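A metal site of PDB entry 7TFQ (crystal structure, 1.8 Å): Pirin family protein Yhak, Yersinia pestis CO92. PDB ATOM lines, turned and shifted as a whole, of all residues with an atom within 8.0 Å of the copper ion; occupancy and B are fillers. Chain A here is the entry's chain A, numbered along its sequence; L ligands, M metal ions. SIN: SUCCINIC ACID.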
ATOM      1  N   VAL A  19      -9.890  -5.805 -21.766  1.00  0.00           N
ATOM      2  CA  VAL A  19     -10.973  -6.735 -22.019  1.00  0.00           C
ATOM      3  C   VAL A  19     -11.446  -7.232 -20.658  1.00  0.00           C
ATOM      4  O   VAL A  19     -10.717  -7.929 -19.950  1.00  0.00           O
ATOM      5  CB  VAL A  19     -10.510  -7.889 -22.911  1.00  0.00           C
ATOM      6  CG1 VAL A  19     -11.591  -8.949 -23.027  1.00  0.00           C
ATOM      7  CG2 VAL A  19     -10.118  -7.329 -24.300  1.00  0.00           C
ATOM      8  N   VAL A  61     -13.173 -11.946 -17.963  1.00  0.00           N
ATOM      9  CA  VAL A  61     -14.128 -11.430 -18.927  1.00  0.00           C
ATOM     10  C   VAL A  61     -15.374 -12.304 -18.824  1.00  0.00           C
ATOM     11  O   VAL A  61     -15.279 -13.537 -18.770  1.00  0.00           O
ATOM     12  CB  VAL A  61     -13.579 -11.397 -20.356  1.00  0.00           C
ATOM     13  CG1 VAL A  61     -13.159 -12.797 -20.845  1.00  0.00           C
ATOM     14  CG2 VAL A  61     -14.591 -10.756 -21.286  1.00  0.00           C
ATOM     15  N   GLY A  62     -16.520 -11.661 -18.758  1.00  0.00           N
ATOM     16  CA  GLY A  62     -17.759 -12.378 -18.588  1.00  0.00           C
ATOM     17  C   GLY A  62     -18.181 -13.105 -19.852  1.00  0.00           C
ATOM     18  O   GLY A  62     -17.587 -12.992 -20.922  1.00  0.00           O
ATOM     19  N   GLN A  63     -19.274 -13.857 -19.698  1.00  0.00           N
ATOM     20  CA  GLN A  63     -19.731 -14.754 -20.752  1.00  0.00           C
ATOM     21  C   GLN A  63     -20.117 -13.992 -22.008  1.00  0.00           C
ATOM     22  O   GLN A  63     -20.817 -12.974 -21.943  1.00  0.00           O
ATOM     23  CB  GLN A  63     -20.917 -15.566 -20.230  1.00  0.00           C
ATOM     24  CG  GLN A  63     -21.520 -16.514 -21.251  1.00  0.00           C
ATOM     25  CD  GLN A  63     -22.843 -17.102 -20.786  1.00  0.00           C
ATOM     26  OE1 GLN A  63     -22.890 -18.230 -20.279  1.00  0.00           O
ATOM     27  NE2 GLN A  63     -23.917 -16.356 -20.958  1.00  0.00           N
ATOM     28  N   HIS A  64     -19.686 -14.497 -23.159  1.00  0.00           N
ATOM     29  CA  HIS A  64     -19.994 -13.877 -24.444  1.00  0.00           C
ATOM     30  C   HIS A  64     -19.871 -14.939 -25.524  1.00  0.00           C
ATOM     31  O   HIS A  64     -19.253 -15.989 -25.311  1.00  0.00           O
ATOM     32  CB  HIS A  64     -19.050 -12.697 -24.735  1.00  0.00           C
ATOM     33  CG  HIS A  64     -17.607 -13.091 -24.749  1.00  0.00           C
ATOM     34  ND1 HIS A  64     -16.865 -13.193 -23.588  1.00  0.00           N
ATOM     35  CD2 HIS A  64     -16.763 -13.396 -25.767  1.00  0.00           C
ATOM     36  CE1 HIS A  64     -15.637 -13.562 -23.888  1.00  0.00           C
ATOM     37  NE2 HIS A  64     -15.538 -13.672 -25.193  1.00  0.00           N
ATOM     38  N   PRO A  65     -20.452 -14.697 -26.704  1.00  0.00           N
ATOM     39  CA  PRO A  65     -20.469 -15.720 -27.745  1.00  0.00           C
ATOM     40  C   PRO A  65     -19.339 -15.575 -28.747  1.00  0.00           C
ATOM     41  O   PRO A  65     -18.761 -14.497 -28.888  1.00  0.00           O
ATOM     42  CB  PRO A  65     -21.808 -15.467 -28.446  1.00  0.00           C
ATOM     43  CG  PRO A  65     -21.897 -13.943 -28.403  1.00  0.00           C
ATOM     44  CD  PRO A  65     -21.320 -13.555 -27.056  1.00  0.00           C
ATOM     45  N   HIS A  66     -19.064 -16.650 -29.482  1.00  0.00           N
ATOM     46  CA  HIS A  66     -18.292 -16.562 -30.711  1.00  0.00           C
ATOM     47  C   HIS A  66     -18.907 -17.519 -31.719  1.00  0.00           C
ATOM     48  O   HIS A  66     -19.560 -18.495 -31.352  1.00  0.00           O
ATOM     49  CB  HIS A  66     -16.830 -16.934 -30.502  1.00  0.00           C
ATOM     50  CG  HIS A  66     -16.082 -15.958 -29.664  1.00  0.00           C
ATOM     51  ND1 HIS A  66     -16.000 -14.620 -29.984  1.00  0.00           N
ATOM     52  CD2 HIS A  66     -15.348 -16.127 -28.539  1.00  0.00           C
ATOM     53  CE1 HIS A  66     -15.281 -13.993 -29.078  1.00  0.00           C
ATOM     54  NE2 HIS A  66     -14.855 -14.889 -28.203  1.00  0.00           N
ATOM     55  N   PHE A  69     -14.845 -19.358 -35.908  1.00  0.00           N
ATOM     56  CA  PHE A  69     -13.382 -19.390 -35.855  1.00  0.00           C
ATOM     57  C   PHE A  69     -12.969 -20.099 -34.569  1.00  0.00           C
ATOM     58  O   PHE A  69     -13.799 -20.697 -33.879  1.00  0.00           O
ATOM     59  CB  PHE A  69     -12.813 -17.959 -35.960  1.00  0.00           C
ATOM     60  CG  PHE A  69     -13.252 -17.042 -34.835  1.00  0.00           C
ATOM     61  CD1 PHE A  69     -14.453 -16.377 -34.905  1.00  0.00           C
ATOM     62  CD2 PHE A  69     -12.450 -16.822 -33.731  1.00  0.00           C
ATOM     63  CE1 PHE A  69     -14.879 -15.546 -33.900  1.00  0.00           C
ATOM     64  CE2 PHE A  69     -12.880 -15.977 -32.707  1.00  0.00           C
ATOM     65  CZ  PHE A  69     -14.108 -15.343 -32.806  1.00  0.00           C
ATOM     66  N   THR A  71     -10.257 -19.860 -30.966  1.00  0.00           N
ATOM     67  CA  THR A  71      -9.429 -18.986 -30.142  1.00  0.00           C
ATOM     68  C   THR A  71      -8.373 -19.832 -29.460  1.00  0.00           C
ATOM     69  O   THR A  71      -8.619 -20.993 -29.103  1.00  0.00           O
ATOM     70  CB  THR A  71     -10.240 -18.185 -29.104  1.00  0.00           C
ATOM     71  OG1 THR A  71     -10.654 -19.043 -28.038  1.00  0.00           O
ATOM     72  CG2 THR A  71     -11.460 -17.537 -29.734  1.00  0.00           C
ATOM     73  N   MET A 100      -9.663 -23.435 -28.471  1.00  0.00           N
ATOM     74  CA  MET A 100     -11.124 -23.555 -28.448  1.00  0.00           C
ATOM     75  C   MET A 100     -11.693 -23.357 -29.825  1.00  0.00           C
ATOM     76  O   MET A 100     -11.378 -22.366 -30.473  1.00  0.00           O
ATOM     77  CB  MET A 100     -11.747 -22.524 -27.493  1.00  0.00           C
ATOM     78  CG  MET A 100     -13.276 -22.573 -27.421  1.00  0.00           C
ATOM     79  SD  MET A 100     -14.028 -21.113 -26.291  1.00  0.00           S
ATOM     80  CE  MET A 100     -13.926 -19.658 -27.522  1.00  0.00           C
ATOM     81  N   ALA A 102     -14.872 -22.350 -31.722  1.00  0.00           N
ATOM     82  CA  ALA A 102     -16.214 -21.789 -31.583  1.00  0.00           C
ATOM     83  C   ALA A 102     -17.152 -22.373 -32.618  1.00  0.00           C
ATOM     84  O   ALA A 102     -18.255 -22.826 -32.287  1.00  0.00           O
ATOM     85  CB  ALA A 102     -16.163 -20.264 -31.686  1.00  0.00           C
ATOM     86  N   ILE A 106     -20.471 -20.884 -29.652  1.00  0.00           N
ATOM     87  CA  ILE A 106     -20.095 -21.240 -28.295  1.00  0.00           C
ATOM     88  C   ILE A 106     -20.257 -20.008 -27.432  1.00  0.00           C
ATOM     89  O   ILE A 106     -20.191 -18.871 -27.915  1.00  0.00           O
ATOM     90  CB  ILE A 106     -18.649 -21.791 -28.249  1.00  0.00           C
ATOM     91  CG1 ILE A 106     -18.450 -22.707 -27.050  1.00  0.00           C
ATOM     92  CG2 ILE A 106     -17.604 -20.633 -28.246  1.00  0.00           C
ATOM     93  CD1 ILE A 106     -17.129 -23.465 -27.102  1.00  0.00           C
ATOM     94  N   LEU A 107     -20.501 -20.217 -26.154  1.00  0.00           N
ATOM     95  CA  LEU A 107     -20.391 -19.184 -25.145  1.00  0.00           C
ATOM     96  C   LEU A 107     -19.194 -19.514 -24.278  1.00  0.00           C
ATOM     97  O   LEU A 107     -18.967 -20.684 -23.949  1.00  0.00           O
ATOM     98  CB  LEU A 107     -21.643 -19.088 -24.264  1.00  0.00           C
ATOM     99  CG  LEU A 107     -22.994 -18.884 -24.905  1.00  0.00           C
ATOM    100  CD1 LEU A 107     -24.101 -18.877 -23.841  1.00  0.00           C
ATOM    101  CD2 LEU A 107     -23.050 -17.582 -25.724  1.00  0.00           C
ATOM    102  N   HIS A 108     -18.413 -18.506 -23.907  1.00  0.00           N
ATOM    103  CA  HIS A 108     -17.352 -18.806 -22.974  1.00  0.00           C
ATOM    104  C   HIS A 108     -17.065 -17.597 -22.095  1.00  0.00           C
ATOM    105  O   HIS A 108     -17.534 -16.483 -22.343  1.00  0.00           O
ATOM    106  CB  HIS A 108     -16.075 -19.295 -23.682  1.00  0.00           C
ATOM    107  CG  HIS A 108     -15.226 -18.201 -24.245  1.00  0.00           C
ATOM    108  ND1 HIS A 108     -13.874 -18.096 -23.974  1.00  0.00           N
ATOM    109  CD2 HIS A 108     -15.520 -17.187 -25.107  1.00  0.00           C
ATOM    110  CE1 HIS A 108     -13.375 -17.053 -24.622  1.00  0.00           C
ATOM    111  NE2 HIS A 108     -14.350 -16.488 -25.319  1.00  0.00           N
ATOM    112  N   GLU A 109     -16.334 -17.869 -21.027  1.00  0.00           N
ATOM    113  CA  GLU A 109     -15.837 -16.877 -20.097  1.00  0.00           C
ATOM    114  C   GLU A 109     -14.467 -17.340 -19.643  1.00  0.00           C
ATOM    115  O   GLU A 109     -14.168 -18.540 -19.672  1.00  0.00           O
ATOM    116  CB  GLU A 109     -16.802 -16.690 -18.908  1.00  0.00           C
ATOM    117  CG  GLU A 109     -16.983 -17.953 -18.106  1.00  0.00           C
ATOM    118  CD  GLU A 109     -18.182 -17.880 -17.149  1.00  0.00           C
ATOM    119  OE1 GLU A 109     -19.225 -17.298 -17.508  1.00  0.00           O
ATOM    120  OE2 GLU A 109     -18.066 -18.425 -16.025  1.00  0.00           O
ATOM    121  N   GLU A 110     -13.627 -16.394 -19.263  1.00  0.00           N
ATOM    122  CA  GLU A 110     -12.243 -16.682 -18.872  1.00  0.00           C
ATOM    123  C   GLU A 110     -11.935 -15.782 -17.693  1.00  0.00           C
ATOM    124  O   GLU A 110     -12.198 -14.581 -17.751  1.00  0.00           O
ATOM    125  CB  GLU A 110     -11.255 -16.391 -20.002  1.00  0.00           C
ATOM    126  CG  GLU A 110     -11.609 -16.969 -21.360  1.00  0.00           C
ATOM    127  CD  GLU A 110     -11.297 -18.451 -21.463  1.00  0.00           C
ATOM    128  OE1 GLU A 110     -10.482 -18.937 -20.643  1.00  0.00           O
ATOM    129  OE2 GLU A 110     -11.850 -19.126 -22.361  1.00  0.00           O
ATOM    130  N   GLN A 127      -3.624 -14.235 -26.699  1.00  0.00           N
ATOM    131  CA  GLN A 127      -4.893 -14.724 -27.216  1.00  0.00           C
ATOM    132  C   GLN A 127      -4.853 -14.561 -28.730  1.00  0.00           C
ATOM    133  O   GLN A 127      -4.652 -13.449 -29.232  1.00  0.00           O
ATOM    134  CB  GLN A 127      -6.056 -13.943 -26.613  1.00  0.00           C
ATOM    135  CG  GLN A 127      -7.418 -14.500 -26.974  1.00  0.00           C
ATOM    136  CD  GLN A 127      -7.755 -15.747 -26.176  1.00  0.00           C
ATOM    137  OE1 GLN A 127      -6.993 -16.161 -25.296  1.00  0.00           O
ATOM    138  NE2 GLN A 127      -8.900 -16.346 -26.468  1.00  0.00           N
ATOM    139  N   TRP A 129      -6.808 -15.446 -32.469  1.00  0.00           N
ATOM    140  CA  TRP A 129      -7.984 -15.974 -33.154  1.00  0.00           C
ATOM    141  C   TRP A 129      -7.487 -16.591 -34.456  1.00  0.00           C
ATOM    142  O   TRP A 129      -6.711 -15.966 -35.175  1.00  0.00           O
ATOM    143  CB  TRP A 129      -9.011 -14.892 -33.489  1.00  0.00           C
ATOM    144  CG  TRP A 129      -9.754 -14.349 -32.330  1.00  0.00           C
ATOM    145  CD1 TRP A 129      -9.567 -14.613 -31.000  1.00  0.00           C
ATOM    146  CD2 TRP A 129     -10.875 -13.460 -32.417  1.00  0.00           C
ATOM    147  NE1 TRP A 129     -10.515 -13.906 -30.247  1.00  0.00           N
ATOM    148  CE2 TRP A 129     -11.317 -13.179 -31.100  1.00  0.00           C
ATOM    149  CE3 TRP A 129     -11.541 -12.856 -33.503  1.00  0.00           C
ATOM    150  CZ2 TRP A 129     -12.412 -12.347 -30.834  1.00  0.00           C
ATOM    151  CZ3 TRP A 129     -12.635 -12.007 -33.224  1.00  0.00           C
ATOM    152  CH2 TRP A 129     -13.049 -11.784 -31.907  1.00  0.00           C
ATOM    153  N   PRO A 265     -17.792 -10.250 -31.911  1.00  0.00           N
ATOM    154  CA  PRO A 265     -17.326 -11.593 -31.567  1.00  0.00           C
ATOM    155  C   PRO A 265     -17.508 -12.640 -32.661  1.00  0.00           C
ATOM    156  O   PRO A 265     -17.232 -13.823 -32.403  1.00  0.00           O
ATOM    157  CB  PRO A 265     -18.219 -11.942 -30.379  1.00  0.00           C
ATOM    158  CG  PRO A 265     -19.515 -11.317 -30.750  1.00  0.00           C
ATOM    159  CD  PRO A 265     -19.131  -9.981 -31.359  1.00  0.00           C
HETATM  160  C1  SIN L   1      -9.050 -11.353 -25.575  1.00  0.00           C
HETATM  161  O1  SIN L   1      -8.007 -10.861 -25.088  1.00  0.00           O
HETATM  162  O2  SIN L   1      -9.414 -10.935 -26.702  1.00  0.00           O
HETATM  163  C2  SIN L   1      -9.811 -12.434 -24.823  1.00  0.00           C
HETATM  164  C3  SIN L   1     -11.333 -12.272 -24.885  1.00  0.00           C
HETATM  165  C4  SIN L   1     -11.946 -13.046 -26.049  1.00  0.00           C
HETATM  166  O3  SIN L   1     -11.869 -14.297 -26.111  1.00  0.00           O
HETATM  167  O4  SIN L   1     -12.544 -12.437 -26.968  1.00  0.00           O
HETATM  168 CU    CU M   1     -14.218 -14.675 -26.343  1.00  0.00          CU
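A ring nitrogen (ND1) of His 66 sits at hydrogen-bond distance from the backbone carbonyl oxygen of Pro 265, 2.8 Å away.
The backbone NH of His 66 lies within hydrogen-bond range of the backbone carbonyl oxygen of Ile 106, at 2.9 Å.
O of Gly 62 sits at hydrogen-bond distance from ND1 of His 64 (2.8 Å).
ND1 of His 108 sits at hydrogen-bond distance from OE2 of Glu 110, at 2.8 Å.
Of the 19 residues printed, 3 come within 4 Å of the copper ion.
The copper ion is bound by a ring nitrogen (NE2) of His 66 (2.0 Å), a ring nitrogen (NE2) of His 64 (2.0 Å), a ring nitrogen (NE2) of His 108 (2.1 Å) and an oxygen (O3) of the ligand (2.4 Å).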
